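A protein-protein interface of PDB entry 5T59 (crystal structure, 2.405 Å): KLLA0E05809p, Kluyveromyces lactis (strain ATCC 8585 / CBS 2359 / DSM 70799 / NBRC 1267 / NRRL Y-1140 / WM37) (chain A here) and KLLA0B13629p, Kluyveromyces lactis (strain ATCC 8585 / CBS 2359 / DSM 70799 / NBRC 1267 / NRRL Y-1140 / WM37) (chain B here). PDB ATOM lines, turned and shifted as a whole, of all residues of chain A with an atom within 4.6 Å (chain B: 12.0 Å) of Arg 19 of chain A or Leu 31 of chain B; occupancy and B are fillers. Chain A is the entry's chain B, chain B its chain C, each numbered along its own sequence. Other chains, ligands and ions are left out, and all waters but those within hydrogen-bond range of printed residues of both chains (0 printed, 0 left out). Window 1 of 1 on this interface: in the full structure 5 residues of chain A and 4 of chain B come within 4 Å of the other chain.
Of chain B, only Met 28 (3.6 Å) comes within 4 Å of Ile 15 of chain A. No residue of chain B comes within 4 Å of Gln 18 of chain A. Arg 19 of chain A touches just these residues of chain B: Met 28 and Leu 31. No residue of chain B comes within 4 Å of Leu 20 of chain A. Gln 22 of chain A touches one residue of chain B. Of chain B, only Leu 31 and Phe 35 come within 4 Å of Val 23 of chain A. Asp 24 of chain B touches none of the printed residues of chain A. Of the printed residues of chain A, Met 28 of chain B touches Ile 15 (3.6 Å) and Arg 19 (3.5 Å). Leu 31 of chain B touches just these residues of chain A: Arg 19, Gln 22 and Val 23. Of the printed residues of chain A, Asn 32 of chain B touches Lys 26 (3.6 Å). Of the printed residues of chain A, Phe 35 of chain B touches Val 23. The nearest printed residue of chain B that does not touch Arg 19 of chain A is Tyr 26 of chain B (4.8 Å).
Of the 18 printed residues of chain B, 4 touch a printed residue of chain A. Printed residues of chain B that touch a printed residue of chain A: Met 28, Leu 31, Asn 32 and Phe 35. Hydrophobic or aromatic side chains of chain B that line the printed part of chain A: Met 28, Leu 31 and Phe 35. Along chain B the printed residues that touch a printed residue of chain A span positions 28 to 35. Of the 10 printed residues of chain A, 5 touch a printed residue of chain B.
Among the printed residues, pairs that only touch across the chains: Arg 19 of chain A with Met 28 of chain B (3.5 Å), Ile 15 of chain A with Met 28 of chain B (3.6 Å), Lys 26 of chain A with Asn 32 of chain B (3.6 Å), Val 23 of chain A with Leu 31 of chain B (3.7 Å), Val 23 of chain A with Phe 35 of chain B (3.8 Å), Gln 22 of chain A with Leu 31 of chain B (3.96 Å) and Arg 19 of chain A with Leu 31 of chain B (3.97 Å).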
ATOM      1  N   ILE A  15      -9.243  25.111 -33.384  1.00  0.00           N
ATOM      2  CA  ILE A  15      -8.955  24.584 -32.050  1.00  0.00           C
ATOM      3  C   ILE A  15      -8.750  23.072 -32.025  1.00  0.00           C
ATOM      4  O   ILE A  15      -8.243  22.545 -31.022  1.00  0.00           O
ATOM      5  CB  ILE A  15     -10.067  24.983 -31.060  1.00  0.00           C
ATOM      6  CG1 ILE A  15     -11.426  24.461 -31.534  1.00  0.00           C
ATOM      7  CG2 ILE A  15     -10.121  26.503 -30.891  1.00  0.00           C
ATOM      8  CD1 ILE A  15     -11.831  23.157 -30.875  1.00  0.00           C
ATOM      9  N   ARG A  16      -9.124  22.320 -33.067  1.00  0.00           N
ATOM     10  CA  ARG A  16      -9.034  20.867 -32.968  1.00  0.00           C
ATOM     11  C   ARG A  16      -7.629  20.346 -33.249  1.00  0.00           C
ATOM     12  O   ARG A  16      -7.208  19.357 -32.647  1.00  0.00           O
ATOM     13  CB  ARG A  16     -10.034  20.208 -33.909  1.00  0.00           C
ATOM     14  CG  ARG A  16      -9.907  18.717 -33.867  1.00  0.00           C
ATOM     15  CD  ARG A  16     -11.068  17.988 -34.499  1.00  0.00           C
ATOM     16  NE  ARG A  16     -12.277  18.002 -33.669  1.00  0.00           N
ATOM     17  CZ  ARG A  16     -13.361  18.742 -33.890  1.00  0.00           C
ATOM     18  NH1 ARG A  16     -13.419  19.565 -34.924  1.00  0.00           N
ATOM     19  NH2 ARG A  16     -14.401  18.659 -33.067  1.00  0.00           N
ATOM     20  N   PHE A  17      -6.910  20.944 -34.202  1.00  0.00           N
ATOM     21  CA  PHE A  17      -5.566  20.446 -34.478  1.00  0.00           C
ATOM     22  C   PHE A  17      -4.638  20.680 -33.292  1.00  0.00           C
ATOM     23  O   PHE A  17      -3.920  19.766 -32.871  1.00  0.00           O
ATOM     24  CB  PHE A  17      -4.982  21.083 -35.734  1.00  0.00           C
ATOM     25  CG  PHE A  17      -3.550  20.696 -35.973  1.00  0.00           C
ATOM     26  CD1 PHE A  17      -3.235  19.448 -36.488  1.00  0.00           C
ATOM     27  CD2 PHE A  17      -2.520  21.568 -35.665  1.00  0.00           C
ATOM     28  CE1 PHE A  17      -1.921  19.080 -36.698  1.00  0.00           C
ATOM     29  CE2 PHE A  17      -1.200  21.208 -35.873  1.00  0.00           C
ATOM     30  CZ  PHE A  17      -0.900  19.962 -36.391  1.00  0.00           C
ATOM     31  N   GLN A  18      -4.635  21.899 -32.738  1.00  0.00           N
ATOM     32  CA  GLN A  18      -3.802  22.161 -31.567  1.00  0.00           C
ATOM     33  C   GLN A  18      -4.042  21.104 -30.499  1.00  0.00           C
ATOM     34  O   GLN A  18      -3.118  20.716 -29.778  1.00  0.00           O
ATOM     35  CB  GLN A  18      -4.075  23.561 -31.006  1.00  0.00           C
ATOM     36  CG  GLN A  18      -5.472  23.756 -30.442  1.00  0.00           C
ATOM     37  CD  GLN A  18      -5.689  25.149 -29.881  1.00  0.00           C
ATOM     38  OE1 GLN A  18      -4.965  26.086 -30.220  1.00  0.00           O
ATOM     39  NE2 GLN A  18      -6.687  25.290 -29.013  1.00  0.00           N
ATOM     40  N   ARG A  19      -5.284  20.626 -30.387  1.00  0.00           N
ATOM     41  CA  ARG A  19      -5.579  19.499 -29.508  1.00  0.00           C
ATOM     42  C   ARG A  19      -4.776  18.269 -29.903  1.00  0.00           C
ATOM     43  O   ARG A  19      -4.162  17.612 -29.054  1.00  0.00           O
ATOM     44  CB  ARG A  19      -7.065  19.155 -29.563  1.00  0.00           C
ATOM     45  CG  ARG A  19      -7.454  17.996 -28.666  1.00  0.00           C
ATOM     46  CD  ARG A  19      -7.359  18.361 -27.207  1.00  0.00           C
ATOM     47  NE  ARG A  19      -8.351  19.383 -26.905  1.00  0.00           N
ATOM     48  CZ  ARG A  19      -8.483  19.989 -25.731  1.00  0.00           C
ATOM     49  NH1 ARG A  19      -7.677  19.680 -24.729  1.00  0.00           N
ATOM     50  NH2 ARG A  19      -9.429  20.904 -25.564  1.00  0.00           N
ATOM     51  N   LEU A  20      -4.820  17.908 -31.185  1.00  0.00           N
ATOM     52  CA  LEU A  20      -4.069  16.752 -31.653  1.00  0.00           C
ATOM     53  C   LEU A  20      -2.610  16.844 -31.226  1.00  0.00           C
ATOM     54  O   LEU A  20      -2.014  15.848 -30.801  1.00  0.00           O
ATOM     55  CB  LEU A  20      -4.197  16.640 -33.168  1.00  0.00           C
ATOM     56  CG  LEU A  20      -3.443  15.483 -33.821  1.00  0.00           C
ATOM     57  CD1 LEU A  20      -3.959  14.169 -33.287  1.00  0.00           C
ATOM     58  CD2 LEU A  20      -3.596  15.554 -35.335  1.00  0.00           C
ATOM     59  N   VAL A  21      -2.015  18.036 -31.328  1.00  0.00           N
ATOM     60  CA  VAL A  21      -0.641  18.214 -30.868  1.00  0.00           C
ATOM     61  C   VAL A  21      -0.566  18.083 -29.351  1.00  0.00           C
ATOM     62  O   VAL A  21       0.418  17.554 -28.818  1.00  0.00           O
ATOM     63  CB  VAL A  21      -0.094  19.570 -31.352  1.00  0.00           C
ATOM     64  CG1 VAL A  21       1.299  19.822 -30.800  1.00  0.00           C
ATOM     65  CG2 VAL A  21      -0.080  19.618 -32.881  1.00  0.00           C
ATOM     66  N   GLN A  22      -1.594  18.543 -28.631  1.00  0.00           N
ATOM     67  CA  GLN A  22      -1.567  18.473 -27.173  1.00  0.00           C
ATOM     68  C   GLN A  22      -1.744  17.045 -26.682  1.00  0.00           C
ATOM     69  O   GLN A  22      -1.138  16.649 -25.681  1.00  0.00           O
ATOM     70  CB  GLN A  22      -2.656  19.366 -26.577  1.00  0.00           C
ATOM     71  CG  GLN A  22      -2.443  20.863 -26.776  1.00  0.00           C
ATOM     72  CD  GLN A  22      -3.609  21.679 -26.251  1.00  0.00           C
ATOM     73  OE1 GLN A  22      -4.732  21.180 -26.143  1.00  0.00           O
ATOM     74  NE2 GLN A  22      -3.350  22.935 -25.910  1.00  0.00           N
ATOM     75  N   VAL A  23      -2.558  16.251 -27.374  1.00  0.00           N
ATOM     76  CA  VAL A  23      -2.792  14.883 -26.924  1.00  0.00           C
ATOM     77  C   VAL A  23      -1.617  13.979 -27.286  1.00  0.00           C
ATOM     78  O   VAL A  23      -1.309  13.037 -26.550  1.00  0.00           O
ATOM     79  CB  VAL A  23      -4.112  14.342 -27.499  1.00  0.00           C
ATOM     80  CG1 VAL A  23      -4.034  14.206 -29.009  1.00  0.00           C
ATOM     81  CG2 VAL A  23      -4.472  13.023 -26.845  1.00  0.00           C
ATOM     82  N   LYS A  26       1.066  14.857 -24.860  1.00  0.00           N
ATOM     83  CA  LYS A  26       0.647  14.383 -23.544  1.00  0.00           C
ATOM     84  C   LYS A  26       0.873  12.882 -23.403  1.00  0.00           C
ATOM     85  O   LYS A  26       1.249  12.402 -22.328  1.00  0.00           O
ATOM     86  CB  LYS A  26      -0.822  14.743 -23.314  1.00  0.00           C
ATOM     87  CG  LYS A  26      -1.336  14.502 -21.905  1.00  0.00           C
ATOM     88  CD  LYS A  26      -0.673  15.466 -20.926  1.00  0.00           C
ATOM     89  CE  LYS A  26      -1.225  15.327 -19.520  1.00  0.00           C
ATOM     90  NZ  LYS A  26      -2.656  15.744 -19.446  1.00  0.00           N
ATOM     91  N   VAL B  17     -13.738   4.052 -21.355  1.00  0.00           N
ATOM     92  CA  VAL B  17     -13.756   5.400 -20.797  1.00  0.00           C
ATOM     93  C   VAL B  17     -14.872   5.478 -19.762  1.00  0.00           C
ATOM     94  O   VAL B  17     -15.816   6.266 -19.893  1.00  0.00           O
ATOM     95  CB  VAL B  17     -13.917   6.467 -21.903  1.00  0.00           C
ATOM     96  CG1 VAL B  17     -15.217   6.276 -22.694  1.00  0.00           C
ATOM     97  CG2 VAL B  17     -13.824   7.878 -21.319  1.00  0.00           C
ATOM     98  N   LYS B  19     -14.997   6.764 -16.896  1.00  0.00           N
ATOM     99  CA  LYS B  19     -14.810   7.825 -15.902  1.00  0.00           C
ATOM    100  C   LYS B  19     -16.000   8.786 -15.895  1.00  0.00           C
ATOM    101  O   LYS B  19     -15.859  10.009 -15.898  1.00  0.00           O
ATOM    102  CB  LYS B  19     -13.494   8.555 -16.166  1.00  0.00           C
ATOM    103  CG  LYS B  19     -13.074   9.566 -15.099  1.00  0.00           C
ATOM    104  CD  LYS B  19     -12.860   8.889 -13.747  1.00  0.00           C
ATOM    105  CE  LYS B  19     -12.063   9.768 -12.797  1.00  0.00           C
ATOM    106  NZ  LYS B  19     -12.742  11.064 -12.532  1.00  0.00           N
ATOM    107  N   VAL B  21     -18.736  11.319 -16.222  1.00  0.00           N
ATOM    108  CA  VAL B  21     -18.973  12.476 -17.084  1.00  0.00           C
ATOM    109  C   VAL B  21     -17.696  13.039 -17.678  1.00  0.00           C
ATOM    110  O   VAL B  21     -17.766  13.945 -18.520  1.00  0.00           O
ATOM    111  CB  VAL B  21     -19.669  13.628 -16.335  1.00  0.00           C
ATOM    112  CG1 VAL B  21     -21.065  13.221 -15.893  1.00  0.00           C
ATOM    113  CG2 VAL B  21     -18.829  14.081 -15.136  1.00  0.00           C
ATOM    114  N   GLN B  22     -16.535  12.540 -17.259  1.00  0.00           N
ATOM    115  CA  GLN B  22     -15.263  13.084 -17.707  1.00  0.00           C
ATOM    116  C   GLN B  22     -15.140  14.510 -17.174  1.00  0.00           C
ATOM    117  O   GLN B  22     -15.196  14.723 -15.959  1.00  0.00           O
ATOM    118  CB  GLN B  22     -15.167  13.032 -19.235  1.00  0.00           C
ATOM    119  CG  GLN B  22     -15.500  11.662 -19.828  1.00  0.00           C
ATOM    120  CD  GLN B  22     -14.632  10.547 -19.296  1.00  0.00           C
ATOM    121  OE1 GLN B  22     -15.076   9.749 -18.473  1.00  0.00           O
ATOM    122  NE2 GLN B  22     -13.385  10.489 -19.754  1.00  0.00           N
ATOM    123  N   LYS B  23     -14.980  15.492 -18.060  1.00  0.00           N
ATOM    124  CA  LYS B  23     -15.042  16.895 -17.668  1.00  0.00           C
ATOM    125  C   LYS B  23     -14.989  17.772 -18.911  1.00  0.00           C
ATOM    126  O   LYS B  23     -13.926  17.935 -19.516  1.00  0.00           O
ATOM    127  CB  LYS B  23     -13.902  17.257 -16.713  1.00  0.00           C
ATOM    128  CG  LYS B  23     -13.971  18.693 -16.217  1.00  0.00           C
ATOM    129  CD  LYS B  23     -12.923  18.977 -15.156  1.00  0.00           C
ATOM    130  CE  LYS B  23     -12.983  20.428 -14.711  1.00  0.00           C
ATOM    131  NZ  LYS B  23     -12.522  21.365 -15.778  1.00  0.00           N
ATOM    132  N   ASP B  24     -16.124  18.341 -19.299  1.00  0.00           N
ATOM    133  CA  ASP B  24     -16.255  19.029 -20.577  1.00  0.00           C
ATOM    134  C   ASP B  24     -16.022  20.523 -20.389  1.00  0.00           C
ATOM    135  O   ASP B  24     -16.701  21.166 -19.582  1.00  0.00           O
ATOM    136  CB  ASP B  24     -17.632  18.772 -21.192  1.00  0.00           C
ATOM    137  CG  ASP B  24     -17.814  17.330 -21.640  1.00  0.00           C
ATOM    138  OD1 ASP B  24     -16.807  16.598 -21.729  1.00  0.00           O
ATOM    139  OD2 ASP B  24     -18.966  16.934 -21.922  1.00  0.00           O
ATOM    140  N   GLU B  25     -15.053  21.062 -21.126  1.00  0.00           N
ATOM    141  CA  GLU B  25     -14.801  22.495 -21.182  1.00  0.00           C
ATOM    142  C   GLU B  25     -14.215  22.812 -22.548  1.00  0.00           C
ATOM    143  O   GLU B  25     -13.526  21.981 -23.146  1.00  0.00           O
ATOM    144  CB  GLU B  25     -13.840  22.958 -20.078  1.00  0.00           C
ATOM    145  CG  GLU B  25     -14.380  22.833 -18.655  1.00  0.00           C
ATOM    146  CD  GLU B  25     -15.639  23.651 -18.423  1.00  0.00           C
ATOM    147  OE1 GLU B  25     -15.724  24.781 -18.950  1.00  0.00           O
ATOM    148  OE2 GLU B  25     -16.542  23.167 -17.708  1.00  0.00           O
ATOM    149  N   TYR B  26     -14.488  24.018 -23.041  1.00  0.00           N
ATOM    150  CA  TYR B  26     -13.991  24.440 -24.349  1.00  0.00           C
ATOM    151  C   TYR B  26     -14.563  23.576 -25.470  1.00  0.00           C
ATOM    152  O   TYR B  26     -13.926  23.383 -26.508  1.00  0.00           O
ATOM    153  CB  TYR B  26     -12.463  24.417 -24.388  1.00  0.00           C
ATOM    154  CG  TYR B  26     -11.811  25.438 -23.487  1.00  0.00           C
ATOM    155  CD1 TYR B  26     -11.401  26.666 -23.984  1.00  0.00           C
ATOM    156  CD2 TYR B  26     -11.645  25.189 -22.130  1.00  0.00           C
ATOM    157  CE1 TYR B  26     -10.807  27.606 -23.164  1.00  0.00           C
ATOM    158  CE2 TYR B  26     -11.055  26.123 -21.301  1.00  0.00           C
ATOM    159  CZ  TYR B  26     -10.640  27.332 -21.824  1.00  0.00           C
ATOM    160  OH  TYR B  26     -10.054  28.268 -21.005  1.00  0.00           O
ATOM    161  N   SER B  27     -15.764  23.040 -25.258  1.00  0.00           N
ATOM    162  CA  SER B  27     -16.478  22.177 -26.197  1.00  0.00           C
ATOM    163  C   SER B  27     -15.859  20.790 -26.330  1.00  0.00           C
ATOM    164  O   SER B  27     -16.284  20.017 -27.193  1.00  0.00           O
ATOM    165  CB  SER B  27     -16.571  22.808 -27.592  1.00  0.00           C
ATOM    166  OG  SER B  27     -15.307  22.855 -28.239  1.00  0.00           O
ATOM    167  N   MET B  28     -14.867  20.449 -25.509  1.00  0.00           N
ATOM    168  CA  MET B  28     -14.307  19.102 -25.485  1.00  0.00           C
ATOM    169  C   MET B  28     -13.985  18.716 -24.051  1.00  0.00           C
ATOM    170  O   MET B  28     -13.938  19.557 -23.152  1.00  0.00           O
ATOM    171  CB  MET B  28     -13.048  18.962 -26.351  1.00  0.00           C
ATOM    172  CG  MET B  28     -13.323  18.904 -27.835  1.00  0.00           C
ATOM    173  SD  MET B  28     -11.832  18.648 -28.818  1.00  0.00           S
ATOM    174  CE  MET B  28     -11.154  20.305 -28.840  1.00  0.00           C
ATOM    175  N   GLU B  29     -13.773  17.421 -23.849  1.00  0.00           N
ATOM    176  CA  GLU B  29     -13.419  16.900 -22.536  1.00  0.00           C
ATOM    177  C   GLU B  29     -11.914  17.011 -22.332  1.00  0.00           C
ATOM    178  O   GLU B  29     -11.128  16.685 -23.226  1.00  0.00           O
ATOM    179  CB  GLU B  29     -13.874  15.448 -22.410  1.00  0.00           C
ATOM    180  CG  GLU B  29     -13.204  14.523 -23.400  1.00  0.00           C
ATOM    181  CD  GLU B  29     -13.841  13.149 -23.443  1.00  0.00           C
ATOM    182  OE1 GLU B  29     -14.583  12.802 -22.504  1.00  0.00           O
ATOM    183  OE2 GLU B  29     -13.607  12.413 -24.423  1.00  0.00           O
ATOM    184  N   ASN B  30     -11.512  17.463 -21.144  1.00  0.00           N
ATOM    185  CA  ASN B  30     -10.131  17.875 -20.941  1.00  0.00           C
ATOM    186  C   ASN B  30      -9.229  16.661 -20.754  1.00  0.00           C
ATOM    187  O   ASN B  30      -9.625  15.642 -20.178  1.00  0.00           O
ATOM    188  CB  ASN B  30     -10.000  18.840 -19.758  1.00  0.00           C
ATOM    189  CG  ASN B  30     -10.190  18.174 -18.409  1.00  0.00           C
ATOM    190  OD1 ASN B  30     -10.685  17.053 -18.308  1.00  0.00           O
ATOM    191  ND2 ASN B  30      -9.780  18.876 -17.357  1.00  0.00           N
ATOM    192  N   LEU B  31      -8.009  16.781 -21.274  1.00  0.00           N
ATOM    193  CA  LEU B  31      -7.049  15.685 -21.231  1.00  0.00           C
ATOM    194  C   LEU B  31      -6.702  15.309 -19.799  1.00  0.00           C
ATOM    195  O   LEU B  31      -6.803  14.140 -19.412  1.00  0.00           O
ATOM    196  CB  LEU B  31      -5.792  16.099 -21.991  1.00  0.00           C
ATOM    197  CG  LEU B  31      -5.969  16.314 -23.492  1.00  0.00           C
ATOM    198  CD1 LEU B  31      -4.748  16.993 -24.079  1.00  0.00           C
ATOM    199  CD2 LEU B  31      -6.198  14.987 -24.176  1.00  0.00           C
ATOM    200  N   ASN B  32      -6.286  16.294 -18.999  1.00  0.00           N
ATOM    201  CA  ASN B  32      -5.775  16.044 -17.657  1.00  0.00           C
ATOM    202  C   ASN B  32      -6.544  14.943 -16.937  1.00  0.00           C
ATOM    203  O   ASN B  32      -5.972  13.921 -16.542  1.00  0.00           O
ATOM    204  CB  ASN B  32      -5.822  17.345 -16.856  1.00  0.00           C
ATOM    205  CG  ASN B  32      -4.857  18.378 -17.386  1.00  0.00           C
ATOM    206  OD1 ASN B  32      -3.653  18.300 -17.147  1.00  0.00           O
ATOM    207  ND2 ASN B  32      -5.379  19.349 -18.122  1.00  0.00           N
ATOM    208  N   ASP B  33      -7.857  15.118 -16.792  1.00  0.00           N
ATOM    209  CA  ASP B  33      -8.658  14.098 -16.127  1.00  0.00           C
ATOM    210  C   ASP B  33      -8.741  12.827 -16.962  1.00  0.00           C
ATOM    211  O   ASP B  33      -8.757  11.721 -16.408  1.00  0.00           O
ATOM    212  CB  ASP B  33     -10.057  14.647 -15.841  1.00  0.00           C
ATOM    213  CG  ASP B  33     -10.914  13.689 -15.025  1.00  0.00           C
ATOM    214  OD1 ASP B  33     -10.436  12.587 -14.682  1.00  0.00           O
ATOM    215  OD2 ASP B  33     -12.072  14.046 -14.719  1.00  0.00           O
ATOM    216  N   PHE B  34      -8.762  12.963 -18.289  1.00  0.00           N
ATOM    217  CA  PHE B  34      -8.966  11.806 -19.153  1.00  0.00           C
ATOM    218  C   PHE B  34      -7.829  10.800 -19.016  1.00  0.00           C
ATOM    219  O   PHE B  34      -8.055   9.585 -19.069  1.00  0.00           O
ATOM    220  CB  PHE B  34      -9.101  12.260 -20.606  1.00  0.00           C
ATOM    221  CG  PHE B  34      -9.469  11.152 -21.549  1.00  0.00           C
ATOM    222  CD1 PHE B  34     -10.797  10.810 -21.740  1.00  0.00           C
ATOM    223  CD2 PHE B  34      -8.494  10.439 -22.225  1.00  0.00           C
ATOM    224  CE1 PHE B  34     -11.152   9.788 -22.600  1.00  0.00           C
ATOM    225  CE2 PHE B  34      -8.840   9.410 -23.085  1.00  0.00           C
ATOM    226  CZ  PHE B  34     -10.173   9.085 -23.273  1.00  0.00           C
ATOM    227  N   PHE B  35      -6.602  11.284 -18.835  1.00  0.00           N
ATOM    228  CA  PHE B  35      -5.406  10.441 -18.776  1.00  0.00           C
ATOM    229  C   PHE B  35      -4.980  10.114 -17.348  1.00  0.00           C
ATOM    230  O   PHE B  35      -3.788  10.150 -17.031  1.00  0.00           O
ATOM    231  CB  PHE B  35      -4.261  11.114 -19.537  1.00  0.00           C
ATOM    232  CG  PHE B  35      -4.376  11.005 -21.034  1.00  0.00           C
ATOM    233  CD1 PHE B  35      -3.814   9.925 -21.700  1.00  0.00           C
ATOM    234  CD2 PHE B  35      -5.057  11.961 -21.772  1.00  0.00           C
ATOM    235  CE1 PHE B  35      -3.912   9.809 -23.074  1.00  0.00           C
ATOM    236  CE2 PHE B  35      -5.161  11.845 -23.147  1.00  0.00           C
ATOM    237  CZ  PHE B  35      -4.589  10.765 -23.799  1.00  0.00           C
ATOM    238  N   LYS B  36      -5.914   9.772 -16.463  1.00  0.00           N
ATOM    239  CA  LYS B  36      -5.528   9.294 -15.137  1.00  0.00           C
ATOM    240  C   LYS B  36      -6.596   8.384 -14.552  1.00  0.00           C
ATOM    241  O   LYS B  36      -7.778   8.721 -14.561  1.00  0.00           O
ATOM    242  CB  LYS B  36      -5.269  10.470 -14.194  1.00  0.00           C
ATOM    243  CG  LYS B  36      -4.650  10.059 -12.867  1.00  0.00           C
ATOM    244  CD  LYS B  36      -4.266  11.268 -12.026  1.00  0.00           C
ATOM    245  CE  LYS B  36      -3.600  10.848 -10.726  1.00  0.00           C
ATOM    246  NZ  LYS B  36      -3.181  12.015  -9.900  1.00  0.00           N
